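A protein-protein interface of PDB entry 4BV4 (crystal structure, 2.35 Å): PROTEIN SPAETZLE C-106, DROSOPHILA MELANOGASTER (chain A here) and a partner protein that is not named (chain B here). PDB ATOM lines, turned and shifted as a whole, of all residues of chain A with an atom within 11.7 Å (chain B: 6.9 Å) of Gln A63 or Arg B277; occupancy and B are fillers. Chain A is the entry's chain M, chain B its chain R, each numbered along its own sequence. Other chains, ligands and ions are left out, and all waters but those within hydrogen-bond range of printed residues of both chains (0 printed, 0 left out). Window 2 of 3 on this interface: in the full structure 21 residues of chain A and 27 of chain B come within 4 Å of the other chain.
O of Phe A61 lies within hydrogen-bond range of NH2 of Arg B277 (2.9 Å). The backbone nitrogen (N) of Pro A62 sits close to the side-chain amide oxygen (OD1) of Asn B275 (3.5 Å). The backbone carbonyl oxygen of Arg B277 lies within hydrogen-bond range of the side-chain amide nitrogen of Gln A63 (3.2 Å). NH2 of Arg B277 sits at hydrogen-bond distance from O of Ala A59 (3.4 Å). The side-chain amide oxygen (OD1) of Asn A60 sits at hydrogen-bond distance from the side-chain amide nitrogen (ND2) of Asn B275 (3.0 Å). ND2 of Asn A60 lies within hydrogen-bond range of OG of Ser B250.
O of Arg B300 sits at hydrogen-bond distance from N of Asn B275 (2.8 Å). The backbone carbonyl oxygen (O) of Asn B252 is in hydrogen-bond range of the backbone NH (N) of Arg B277, at 2.9 Å. The backbone carbonyl oxygen (O) of Asn B275 sits at hydrogen-bond distance from the guanidinium group (NE) of Arg B277. The backbone NH (N) of Met B274 is in hydrogen-bond range of the side-chain hydroxyl (OG) of Ser B250 (3.1 Å). O of Ser B250 sits at hydrogen-bond distance from ND2 of Asn B252 (2.9 Å). The backbone carbonyl oxygen (O) of Ser B250 lies within hydrogen-bond range of the backbone NH (N) of Asp B227.
Among the printed residues, pairs that only touch across the chains: Ala A59 with Asp B227, Ala A59 with Ala B251, Asn A60 with Met B274, Phe A61 with Asn B275 and Pro A62 with Arg B277.
Of the printed residues of chain B, Ala A59 touches Asp B227, Ala B251 and Arg B277. Of the printed residues of chain B, Phe A61 touches Asn B275 and Arg B277. Gln A63 touches just one residue of chain B: Arg B277 (3.2 Å). Asn A66 touches none of the printed residues of chain B. Of the printed residues of chain A, Asp B227 touches Ala A59 (3.8 Å). Printed residues of chain A within 4 Å of Ser B250: Asn A60. Ala B251 touches just one residue of chain A: Ala A59 (3.5 Å). No residue of chain A comes within 4 Å of Leu B253. Printed residues of chain A within 4 Å of Met B274: Asn A60 (3.6 Å). Asn B276 touches none of the printed residues of chain A. Of chain A, only Ala A59, Phe A61, Pro A62 and Gln A63 come within 4 Å of Arg B277. No residue of chain A comes within 4 Å of Val B278. No residue of chain A comes within 4 Å of Pro B279. The nearest residue of chain B that does not touch Gln A63 is Asn B276 (4.7 Å).
Of the 16 printed residues of chain B, 6 touch a printed residue of chain A. Printed residues of chain B that touch a printed residue of chain A: Asp B227, Ser B250, Ala B251, Met B274, Asn B275 and Arg B277.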
ATOM      1  N   CYS A  55     -14.795   1.214   1.479  1.00  0.00           N
ATOM      2  CA  CYS A  55     -13.941   0.428   0.597  1.00  0.00           C
ATOM      3  C   CYS A  55     -14.808  -0.315  -0.415  1.00  0.00           C
ATOM      4  O   CYS A  55     -15.977  -0.604  -0.144  1.00  0.00           O
ATOM      5  CB  CYS A  55     -13.098  -0.562   1.392  1.00  0.00           C
ATOM      6  SG  CYS A  55     -12.225   0.142   2.808  1.00  0.00           S
ATOM      7  N   PHE A  57     -15.319  -3.966  -2.735  1.00  0.00           N
ATOM      8  CA  PHE A  57     -15.145  -5.426  -2.513  1.00  0.00           C
ATOM      9  C   PHE A  57     -15.152  -5.760  -1.008  1.00  0.00           C
ATOM     10  O   PHE A  57     -14.513  -6.714  -0.574  1.00  0.00           O
ATOM     11  CB  PHE A  57     -13.861  -5.966  -3.199  1.00  0.00           C
ATOM     12  CG  PHE A  57     -13.634  -5.446  -4.603  1.00  0.00           C
ATOM     13  CD1 PHE A  57     -14.294  -6.012  -5.688  1.00  0.00           C
ATOM     14  CD2 PHE A  57     -12.770  -4.378  -4.838  1.00  0.00           C
ATOM     15  CE1 PHE A  57     -14.109  -5.512  -6.979  1.00  0.00           C
ATOM     16  CE2 PHE A  57     -12.598  -3.872  -6.126  1.00  0.00           C
ATOM     17  CZ  PHE A  57     -13.270  -4.440  -7.189  1.00  0.00           C
ATOM     18  N   ALA A  58     -15.913  -4.983  -0.230  1.00  0.00           N
ATOM     19  CA  ALA A  58     -16.006  -5.095   1.216  1.00  0.00           C
ATOM     20  C   ALA A  58     -17.432  -5.448   1.700  1.00  0.00           C
ATOM     21  O   ALA A  58     -17.757  -5.221   2.865  1.00  0.00           O
ATOM     22  CB  ALA A  58     -15.550  -3.784   1.839  1.00  0.00           C
ATOM     23  N   ALA A  59     -18.257  -6.040   0.832  1.00  0.00           N
ATOM     24  CA  ALA A  59     -19.643  -6.387   1.167  1.00  0.00           C
ATOM     25  C   ALA A  59     -19.783  -7.674   1.998  1.00  0.00           C
ATOM     26  O   ALA A  59     -20.868  -7.930   2.493  1.00  0.00           O
ATOM     27  CB  ALA A  59     -20.451  -6.525  -0.101  1.00  0.00           C
ATOM     28  N   ASN A  60     -18.708  -8.490   2.133  1.00  0.00           N
ATOM     29  CA  ASN A  60     -18.758  -9.747   2.876  1.00  0.00           C
ATOM     30  C   ASN A  60     -17.825  -9.722   4.105  1.00  0.00           C
ATOM     31  O   ASN A  60     -17.014 -10.628   4.315  1.00  0.00           O
ATOM     32  CB  ASN A  60     -18.455 -10.944   1.964  1.00  0.00           C
ATOM     33  CG  ASN A  60     -18.639 -12.291   2.624  1.00  0.00           C
ATOM     34  OD1 ASN A  60     -19.317 -12.423   3.643  1.00  0.00           O
ATOM     35  ND2 ASN A  60     -18.013 -13.320   2.077  1.00  0.00           N
ATOM     36  N   PHE A  61     -18.000  -8.709   4.950  1.00  0.00           N
ATOM     37  CA  PHE A  61     -17.271  -8.585   6.211  1.00  0.00           C
ATOM     38  C   PHE A  61     -18.285  -8.587   7.346  1.00  0.00           C
ATOM     39  O   PHE A  61     -19.452  -8.303   7.073  1.00  0.00           O
ATOM     40  CB  PHE A  61     -16.398  -7.316   6.215  1.00  0.00           C
ATOM     41  CG  PHE A  61     -15.126  -7.511   5.430  1.00  0.00           C
ATOM     42  CD1 PHE A  61     -15.089  -7.265   4.062  1.00  0.00           C
ATOM     43  CD2 PHE A  61     -13.975  -7.978   6.050  1.00  0.00           C
ATOM     44  CE1 PHE A  61     -13.924  -7.481   3.333  1.00  0.00           C
ATOM     45  CE2 PHE A  61     -12.805  -8.179   5.323  1.00  0.00           C
ATOM     46  CZ  PHE A  61     -12.790  -7.940   3.969  1.00  0.00           C
ATOM     47  N   PRO A  62     -17.919  -8.909   8.613  1.00  0.00           N
ATOM     48  CA  PRO A  62     -18.938  -8.922   9.686  1.00  0.00           C
ATOM     49  C   PRO A  62     -19.549  -7.536   9.918  1.00  0.00           C
ATOM     50  O   PRO A  62     -18.907  -6.518   9.638  1.00  0.00           O
ATOM     51  CB  PRO A  62     -18.163  -9.414  10.917  1.00  0.00           C
ATOM     52  CG  PRO A  62     -16.977 -10.106  10.376  1.00  0.00           C
ATOM     53  CD  PRO A  62     -16.609  -9.347   9.128  1.00  0.00           C
ATOM     54  N   GLN A  63     -20.808  -7.509  10.405  1.00  0.00           N
ATOM     55  CA  GLN A  63     -21.603  -6.313  10.703  1.00  0.00           C
ATOM     56  C   GLN A  63     -20.825  -5.284  11.518  1.00  0.00           C
ATOM     57  O   GLN A  63     -20.875  -4.108  11.188  1.00  0.00           O
ATOM     58  CB  GLN A  63     -22.874  -6.683  11.469  1.00  0.00           C
ATOM     59  CG  GLN A  63     -23.954  -7.406  10.664  1.00  0.00           C
ATOM     60  CD  GLN A  63     -25.200  -7.618  11.498  1.00  0.00           C
ATOM     61  OE1 GLN A  63     -25.539  -6.801  12.360  1.00  0.00           O
ATOM     62  NE2 GLN A  63     -25.918  -8.715  11.259  1.00  0.00           N
ATOM     63  N   SER A  64     -20.051  -5.731  12.525  1.00  0.00           N
ATOM     64  CA  SER A  64     -19.242  -4.886  13.404  1.00  0.00           C
ATOM     65  C   SER A  64     -18.205  -4.050  12.647  1.00  0.00           C
ATOM     66  O   SER A  64     -17.826  -2.977  13.130  1.00  0.00           O
ATOM     67  CB  SER A  64     -18.526  -5.747  14.437  1.00  0.00           C
ATOM     68  OG  SER A  64     -17.787  -4.950  15.352  1.00  0.00           O
ATOM     69  N   TYR A  65     -17.718  -4.544  11.496  1.00  0.00           N
ATOM     70  CA  TYR A  65     -16.705  -3.839  10.730  1.00  0.00           C
ATOM     71  C   TYR A  65     -17.321  -2.820   9.762  1.00  0.00           C
ATOM     72  O   TYR A  65     -18.310  -3.111   9.081  1.00  0.00           O
ATOM     73  CB  TYR A  65     -15.808  -4.831   9.958  1.00  0.00           C
ATOM     74  CG  TYR A  65     -14.860  -5.641  10.816  1.00  0.00           C
ATOM     75  CD1 TYR A  65     -13.858  -5.024  11.562  1.00  0.00           C
ATOM     76  CD2 TYR A  65     -14.922  -7.029  10.834  1.00  0.00           C
ATOM     77  CE1 TYR A  65     -12.962  -5.769  12.331  1.00  0.00           C
ATOM     78  CE2 TYR A  65     -14.036  -7.787  11.603  1.00  0.00           C
ATOM     79  CZ  TYR A  65     -13.049  -7.152  12.342  1.00  0.00           C
ATOM     80  OH  TYR A  65     -12.160  -7.890  13.089  1.00  0.00           O
ATOM     81  N   ASN A  66     -16.707  -1.634   9.692  1.00  0.00           N
ATOM     82  CA  ASN A  66     -17.088  -0.566   8.784  1.00  0.00           C
ATOM     83  C   ASN A  66     -15.874  -0.295   7.891  1.00  0.00           C
ATOM     84  O   ASN A  66     -14.996   0.483   8.277  1.00  0.00           O
ATOM     85  CB  ASN A  66     -17.571   0.691   9.545  1.00  0.00           C
ATOM     86  CG  ASN A  66     -18.016   1.848   8.663  1.00  0.00           C
ATOM     87  OD1 ASN A  66     -18.358   1.692   7.479  1.00  0.00           O
ATOM     88  ND2 ASN A  66     -18.033   3.046   9.234  1.00  0.00           N
ATOM     89  N   PRO A  67     -15.742  -1.001   6.742  1.00  0.00           N
ATOM     90  CA  PRO A  67     -14.561  -0.779   5.891  1.00  0.00           C
ATOM     91  C   PRO A  67     -14.598   0.615   5.283  1.00  0.00           C
ATOM     92  O   PRO A  67     -15.477   0.946   4.484  1.00  0.00           O
ATOM     93  CB  PRO A  67     -14.634  -1.891   4.832  1.00  0.00           C
ATOM     94  CG  PRO A  67     -15.766  -2.752   5.223  1.00  0.00           C
ATOM     95  CD  PRO A  67     -16.659  -1.980   6.133  1.00  0.00           C
ATOM     96  N   ILE A  68     -13.642   1.449   5.705  1.00  0.00           N
ATOM     97  CA  ILE A  68     -13.529   2.836   5.271  1.00  0.00           C
ATOM     98  C   ILE A  68     -12.126   3.087   4.747  1.00  0.00           C
ATOM     99  O   ILE A  68     -11.154   2.642   5.353  1.00  0.00           O
ATOM    100  CB  ILE A  68     -13.908   3.795   6.449  1.00  0.00           C
ATOM    101  CG1 ILE A  68     -15.421   3.753   6.790  1.00  0.00           C
ATOM    102  CG2 ILE A  68     -13.410   5.239   6.246  1.00  0.00           C
ATOM    103  CD1 ILE A  68     -16.472   4.090   5.710  1.00  0.00           C
ATOM    104  N   ALA A 103      -9.440   0.627   6.106  1.00  0.00           N
ATOM    105  CA  ALA A 103      -9.440   0.416   7.550  1.00  0.00           C
ATOM    106  C   ALA A 103     -10.740  -0.241   7.968  1.00  0.00           C
ATOM    107  O   ALA A 103     -11.811   0.288   7.685  1.00  0.00           O
ATOM    108  CB  ALA A 103      -9.242   1.732   8.281  1.00  0.00           C
ATOM    109  N   LEU A 104     -10.659  -1.448   8.534  1.00  0.00           N
ATOM    110  CA  LEU A 104     -11.829  -2.146   9.060  1.00  0.00           C
ATOM    111  C   LEU A 104     -12.017  -1.577  10.445  1.00  0.00           C
ATOM    112  O   LEU A 104     -11.277  -1.937  11.369  1.00  0.00           O
ATOM    113  CB  LEU A 104     -11.660  -3.680   9.069  1.00  0.00           C
ATOM    114  CG  LEU A 104     -11.201  -4.392   7.797  1.00  0.00           C
ATOM    115  CD1 LEU A 104     -10.712  -5.804   8.132  1.00  0.00           C
ATOM    116  CD2 LEU A 104     -12.308  -4.470   6.770  1.00  0.00           C
ATOM    117  N   LYS A 105     -12.892  -0.563  10.545  1.00  0.00           N
ATOM    118  CA  LYS A 105     -13.174   0.182  11.779  1.00  0.00           C
ATOM    119  C   LYS A 105     -14.250  -0.522  12.605  1.00  0.00           C
ATOM    120  O   LYS A 105     -15.309  -0.867  12.079  1.00  0.00           O
ATOM    121  CB  LYS A 105     -13.581   1.635  11.459  1.00  0.00           C
ATOM    122  CG  LYS A 105     -12.434   2.485  10.893  1.00  0.00           C
ATOM    123  CD  LYS A 105     -12.920   3.804  10.307  1.00  0.00           C
ATOM    124  CE  LYS A 105     -12.937   4.930  11.318  1.00  0.00           C
ATOM    125  NZ  LYS A 105     -13.578   6.163  10.778  1.00  0.00           N
ATOM    126  N   THR A 106     -13.952  -0.764  13.890  1.00  0.00           N
ATOM    127  CA  THR A 106     -14.838  -1.456  14.832  1.00  0.00           C
ATOM    128  C   THR A 106     -15.697  -0.450  15.594  1.00  0.00           C
ATOM    129  O   THR A 106     -16.919  -0.582  15.625  1.00  0.00           O
ATOM    130  CB  THR A 106     -14.016  -2.323  15.798  1.00  0.00           C
ATOM    131  OG1 THR A 106     -13.174  -1.480  16.588  1.00  0.00           O
ATOM    132  CG2 THR A 106     -13.179  -3.384  15.076  1.00  0.00           C
ATOM    133  N   ASP B 227     -24.476 -10.695  -0.614  1.00  0.00           N
ATOM    134  CA  ASP B 227     -25.101  -9.394  -0.339  1.00  0.00           C
ATOM    135  C   ASP B 227     -26.194  -9.085  -1.377  1.00  0.00           C
ATOM    136  O   ASP B 227     -26.132  -8.088  -2.084  1.00  0.00           O
ATOM    137  CB  ASP B 227     -24.049  -8.249  -0.246  1.00  0.00           C
ATOM    138  CG  ASP B 227     -24.620  -6.871   0.071  1.00  0.00           C
ATOM    139  OD1 ASP B 227     -25.522  -6.786   0.917  1.00  0.00           O
ATOM    140  OD2 ASP B 227     -24.165  -5.883  -0.539  1.00  0.00           O
ATOM    141  N   SER B 250     -22.909 -15.721   0.748  1.00  0.00           N
ATOM    142  CA  SER B 250     -22.594 -14.925   1.926  1.00  0.00           C
ATOM    143  C   SER B 250     -23.412 -13.638   2.056  1.00  0.00           C
ATOM    144  O   SER B 250     -24.118 -13.249   1.129  1.00  0.00           O
ATOM    145  CB  SER B 250     -21.114 -14.585   1.934  1.00  0.00           C
ATOM    146  OG  SER B 250     -20.308 -15.753   1.882  1.00  0.00           O
ATOM    147  N   ALA B 251     -23.342 -13.010   3.255  1.00  0.00           N
ATOM    148  CA  ALA B 251     -23.918 -11.717   3.639  1.00  0.00           C
ATOM    149  C   ALA B 251     -25.372 -11.550   3.166  1.00  0.00           C
ATOM    150  O   ALA B 251     -25.803 -10.453   2.771  1.00  0.00           O
ATOM    151  CB  ALA B 251     -23.032 -10.591   3.112  1.00  0.00           C
ATOM    152  N   ASN B 252     -26.145 -12.655   3.251  1.00  0.00           N
ATOM    153  CA  ASN B 252     -27.562 -12.681   2.899  1.00  0.00           C
ATOM    154  C   ASN B 252     -28.397 -12.808   4.182  1.00  0.00           C
ATOM    155  O   ASN B 252     -27.859 -12.586   5.266  1.00  0.00           O
ATOM    156  CB  ASN B 252     -27.857 -13.764   1.858  1.00  0.00           C
ATOM    157  CG  ASN B 252     -27.494 -13.315   0.452  1.00  0.00           C
ATOM    158  OD1 ASN B 252     -27.988 -12.302  -0.055  1.00  0.00           O
ATOM    159  ND2 ASN B 252     -26.599 -14.028  -0.204  1.00  0.00           N
ATOM    160  N   LEU B 253     -29.718 -13.068   4.064  1.00  0.00           N
ATOM    161  CA  LEU B 253     -30.647 -13.072   5.192  1.00  0.00           C
ATOM    162  C   LEU B 253     -31.405 -14.397   5.357  1.00  0.00           C
ATOM    163  O   LEU B 253     -32.591 -14.379   5.692  1.00  0.00           O
ATOM    164  CB  LEU B 253     -31.664 -11.914   4.986  1.00  0.00           C
ATOM    165  CG  LEU B 253     -31.103 -10.494   4.866  1.00  0.00           C
ATOM    166  CD1 LEU B 253     -32.078  -9.588   4.137  1.00  0.00           C
ATOM    167  CD2 LEU B 253     -30.781  -9.917   6.223  1.00  0.00           C
ATOM    168  N   PHE B 254     -30.741 -15.535   5.159  1.00  0.00           N
ATOM    169  CA  PHE B 254     -31.396 -16.831   5.311  1.00  0.00           C
ATOM    170  C   PHE B 254     -31.692 -17.188   6.771  1.00  0.00           C
ATOM    171  O   PHE B 254     -30.828 -17.057   7.642  1.00  0.00           O
ATOM    172  CB  PHE B 254     -30.554 -17.950   4.713  1.00  0.00           C
ATOM    173  CG  PHE B 254     -30.070 -17.735   3.305  1.00  0.00           C
ATOM    174  CD1 PHE B 254     -30.920 -17.940   2.223  1.00  0.00           C
ATOM    175  CD2 PHE B 254     -28.736 -17.438   3.052  1.00  0.00           C
ATOM    176  CE1 PHE B 254     -30.454 -17.804   0.917  1.00  0.00           C
ATOM    177  CE2 PHE B 254     -28.273 -17.294   1.743  1.00  0.00           C
ATOM    178  CZ  PHE B 254     -29.134 -17.469   0.684  1.00  0.00           C
ATOM    179  N   ARG B 255     -32.928 -17.649   7.015  1.00  0.00           N
ATOM    180  CA  ARG B 255     -33.402 -18.170   8.293  1.00  0.00           C
ATOM    181  C   ARG B 255     -33.383 -19.687   8.182  1.00  0.00           C
ATOM    182  O   ARG B 255     -33.369 -20.380   9.204  1.00  0.00           O
ATOM    183  CB  ARG B 255     -34.799 -17.641   8.647  1.00  0.00           C
ATOM    184  CG  ARG B 255     -34.835 -16.134   8.895  1.00  0.00           C
ATOM    185  CD  ARG B 255     -35.058 -15.792  10.357  1.00  0.00           C
ATOM    186  NE  ARG B 255     -34.947 -14.349  10.594  1.00  0.00           N
ATOM    187  CZ  ARG B 255     -34.597 -13.801  11.756  1.00  0.00           C
ATOM    188  NH1 ARG B 255     -34.321 -14.568  12.806  1.00  0.00           N
ATOM    189  NH2 ARG B 255     -34.506 -12.482  11.871  1.00  0.00           N
ATOM    190  N   MET B 274     -21.018 -17.106   4.626  1.00  0.00           N
ATOM    191  CA  MET B 274     -20.440 -16.348   5.723  1.00  0.00           C
ATOM    192  C   MET B 274     -21.223 -15.078   5.983  1.00  0.00           C
ATOM    193  O   MET B 274     -21.858 -14.530   5.071  1.00  0.00           O
ATOM    194  CB  MET B 274     -18.973 -15.959   5.404  1.00  0.00           C
ATOM    195  CG  MET B 274     -18.092 -17.097   4.993  1.00  0.00           C
ATOM    196  SD  MET B 274     -16.759 -16.504   3.914  1.00  0.00           S
ATOM    197  CE  MET B 274     -15.768 -15.534   5.080  1.00  0.00           C
ATOM    198  N   ASN B 275     -21.116 -14.572   7.226  1.00  0.00           N
ATOM    199  CA  ASN B 275     -21.692 -13.297   7.660  1.00  0.00           C
ATOM    200  C   ASN B 275     -23.136 -13.151   7.277  1.00  0.00           C
ATOM    201  O   ASN B 275     -23.525 -12.114   6.753  1.00  0.00           O
ATOM    202  CB  ASN B 275     -20.874 -12.116   7.105  1.00  0.00           C
ATOM    203  CG  ASN B 275     -19.434 -12.232   7.482  1.00  0.00           C
ATOM    204  OD1 ASN B 275     -19.085 -12.194   8.657  1.00  0.00           O
ATOM    205  ND2 ASN B 275     -18.595 -12.537   6.516  1.00  0.00           N
ATOM    206  N   ASN B 276     -23.946 -14.190   7.560  1.00  0.00           N
ATOM    207  CA  ASN B 276     -25.403 -14.171   7.387  1.00  0.00           C
ATOM    208  C   ASN B 276     -25.896 -13.097   8.344  1.00  0.00           C
ATOM    209  O   ASN B 276     -25.387 -13.006   9.465  1.00  0.00           O
ATOM    210  CB  ASN B 276     -25.980 -15.550   7.679  1.00  0.00           C
ATOM    211  CG  ASN B 276     -27.335 -15.773   7.079  1.00  0.00           C
ATOM    212  OD1 ASN B 276     -27.501 -15.816   5.854  1.00  0.00           O
ATOM    213  ND2 ASN B 276     -28.329 -15.961   7.936  1.00  0.00           N
ATOM    214  N   ARG B 277     -26.760 -12.197   7.877  1.00  0.00           N
ATOM    215  CA  ARG B 277     -27.135 -11.018   8.664  1.00  0.00           C
ATOM    216  C   ARG B 277     -28.209 -11.255   9.720  1.00  0.00           C
ATOM    217  O   ARG B 277     -28.518 -10.338  10.487  1.00  0.00           O
ATOM    218  CB  ARG B 277     -27.531  -9.883   7.735  1.00  0.00           C
ATOM    219  CG  ARG B 277     -26.462  -9.565   6.677  1.00  0.00           C
ATOM    220  CD  ARG B 277     -25.120  -9.210   7.297  1.00  0.00           C
ATOM    221  NE  ARG B 277     -24.087  -8.932   6.299  1.00  0.00           N
ATOM    222  CZ  ARG B 277     -22.817  -8.684   6.596  1.00  0.00           C
ATOM    223  NH1 ARG B 277     -22.405  -8.707   7.857  1.00  0.00           N
ATOM    224  NH2 ARG B 277     -21.943  -8.435   5.634  1.00  0.00           N
ATOM    225  N   VAL B 278     -28.732 -12.492   9.795  1.00  0.00           N
ATOM    226  CA  VAL B 278     -29.761 -12.969  10.738  1.00  0.00           C
ATOM    227  C   VAL B 278     -29.346 -14.373  11.228  1.00  0.00           C
ATOM    228  O   VAL B 278     -28.559 -15.029  10.539  1.00  0.00           O
ATOM    229  CB  VAL B 278     -31.195 -12.973  10.125  1.00  0.00           C
ATOM    230  CG1 VAL B 278     -31.670 -11.564   9.799  1.00  0.00           C
ATOM    231  CG2 VAL B 278     -31.293 -13.882   8.904  1.00  0.00           C
ATOM    232  N   PRO B 279     -29.841 -14.879  12.382  1.00  0.00           N
ATOM    233  CA  PRO B 279     -29.452 -16.228  12.797  1.00  0.00           C
ATOM    234  C   PRO B 279     -30.023 -17.306  11.876  1.00  0.00           C
ATOM    235  O   PRO B 279     -31.213 -17.298  11.558  1.00  0.00           O
ATOM    236  CB  PRO B 279     -30.039 -16.346  14.217  1.00  0.00           C
ATOM    237  CG  PRO B 279     -30.334 -14.952  14.647  1.00  0.00           C
ATOM    238  CD  PRO B 279     -30.759 -14.284  13.374  1.00  0.00           C
ATOM    239  N   ARG B 300     -20.590 -19.315   8.421  1.00  0.00           N
ATOM    240  CA  ARG B 300     -20.745 -18.308   9.480  1.00  0.00           C
ATOM    241  C   ARG B 300     -22.012 -17.438   9.185  1.00  0.00           C
ATOM    242  O   ARG B 300     -22.164 -17.014   8.050  1.00  0.00           O
ATOM    243  CB  ARG B 300     -19.463 -17.443   9.510  1.00  0.00           C
ATOM    244  CG  ARG B 300     -19.273 -16.659  10.776  1.00  0.00           C
ATOM    245  CD  ARG B 300     -18.378 -15.472  10.553  1.00  0.00           C
ATOM    246  NE  ARG B 300     -18.607 -14.462  11.581  1.00  0.00           N
ATOM    247  CZ  ARG B 300     -17.641 -13.774  12.176  1.00  0.00           C
ATOM    248  NH1 ARG B 300     -16.372 -13.981  11.851  1.00  0.00           N
ATOM    249  NH2 ARG B 300     -17.936 -12.878  13.109  1.00  0.00           N
ATOM    250  N   ALA B 301     -22.964 -17.220  10.118  1.00  0.00           N
ATOM    251  CA  ALA B 301     -22.946 -17.552  11.533  1.00  0.00           C
ATOM    252  C   ALA B 301     -24.337 -17.764  12.149  1.00  0.00           C
ATOM    253  O   ALA B 301     -25.385 -17.835  11.483  1.00  0.00           O
ATOM    254  CB  ALA B 301     -22.231 -16.444  12.322  1.00  0.00           C
ATOM    255  N   GLU B 302     -24.269 -17.866  13.484  1.00  0.00           N
ATOM    256  CA  GLU B 302     -25.297 -18.065  14.473  1.00  0.00           C
ATOM    257  C   GLU B 302     -25.924 -19.474  14.325  1.00  0.00           C
ATOM    258  O   GLU B 302     -26.976 -19.737  14.896  1.00  0.00           O
ATOM    259  CB  GLU B 302     -26.286 -16.901  14.452  1.00  0.00           C
ATOM    260  CG  GLU B 302     -25.592 -15.586  14.792  1.00  0.00           C
ATOM    261  CD  GLU B 302     -26.263 -14.335  14.261  1.00  0.00           C
ATOM    262  OE1 GLU B 302     -26.240 -14.116  13.026  1.00  0.00           O
ATOM    263  OE2 GLU B 302     -26.791 -13.557  15.087  1.00  0.00           O
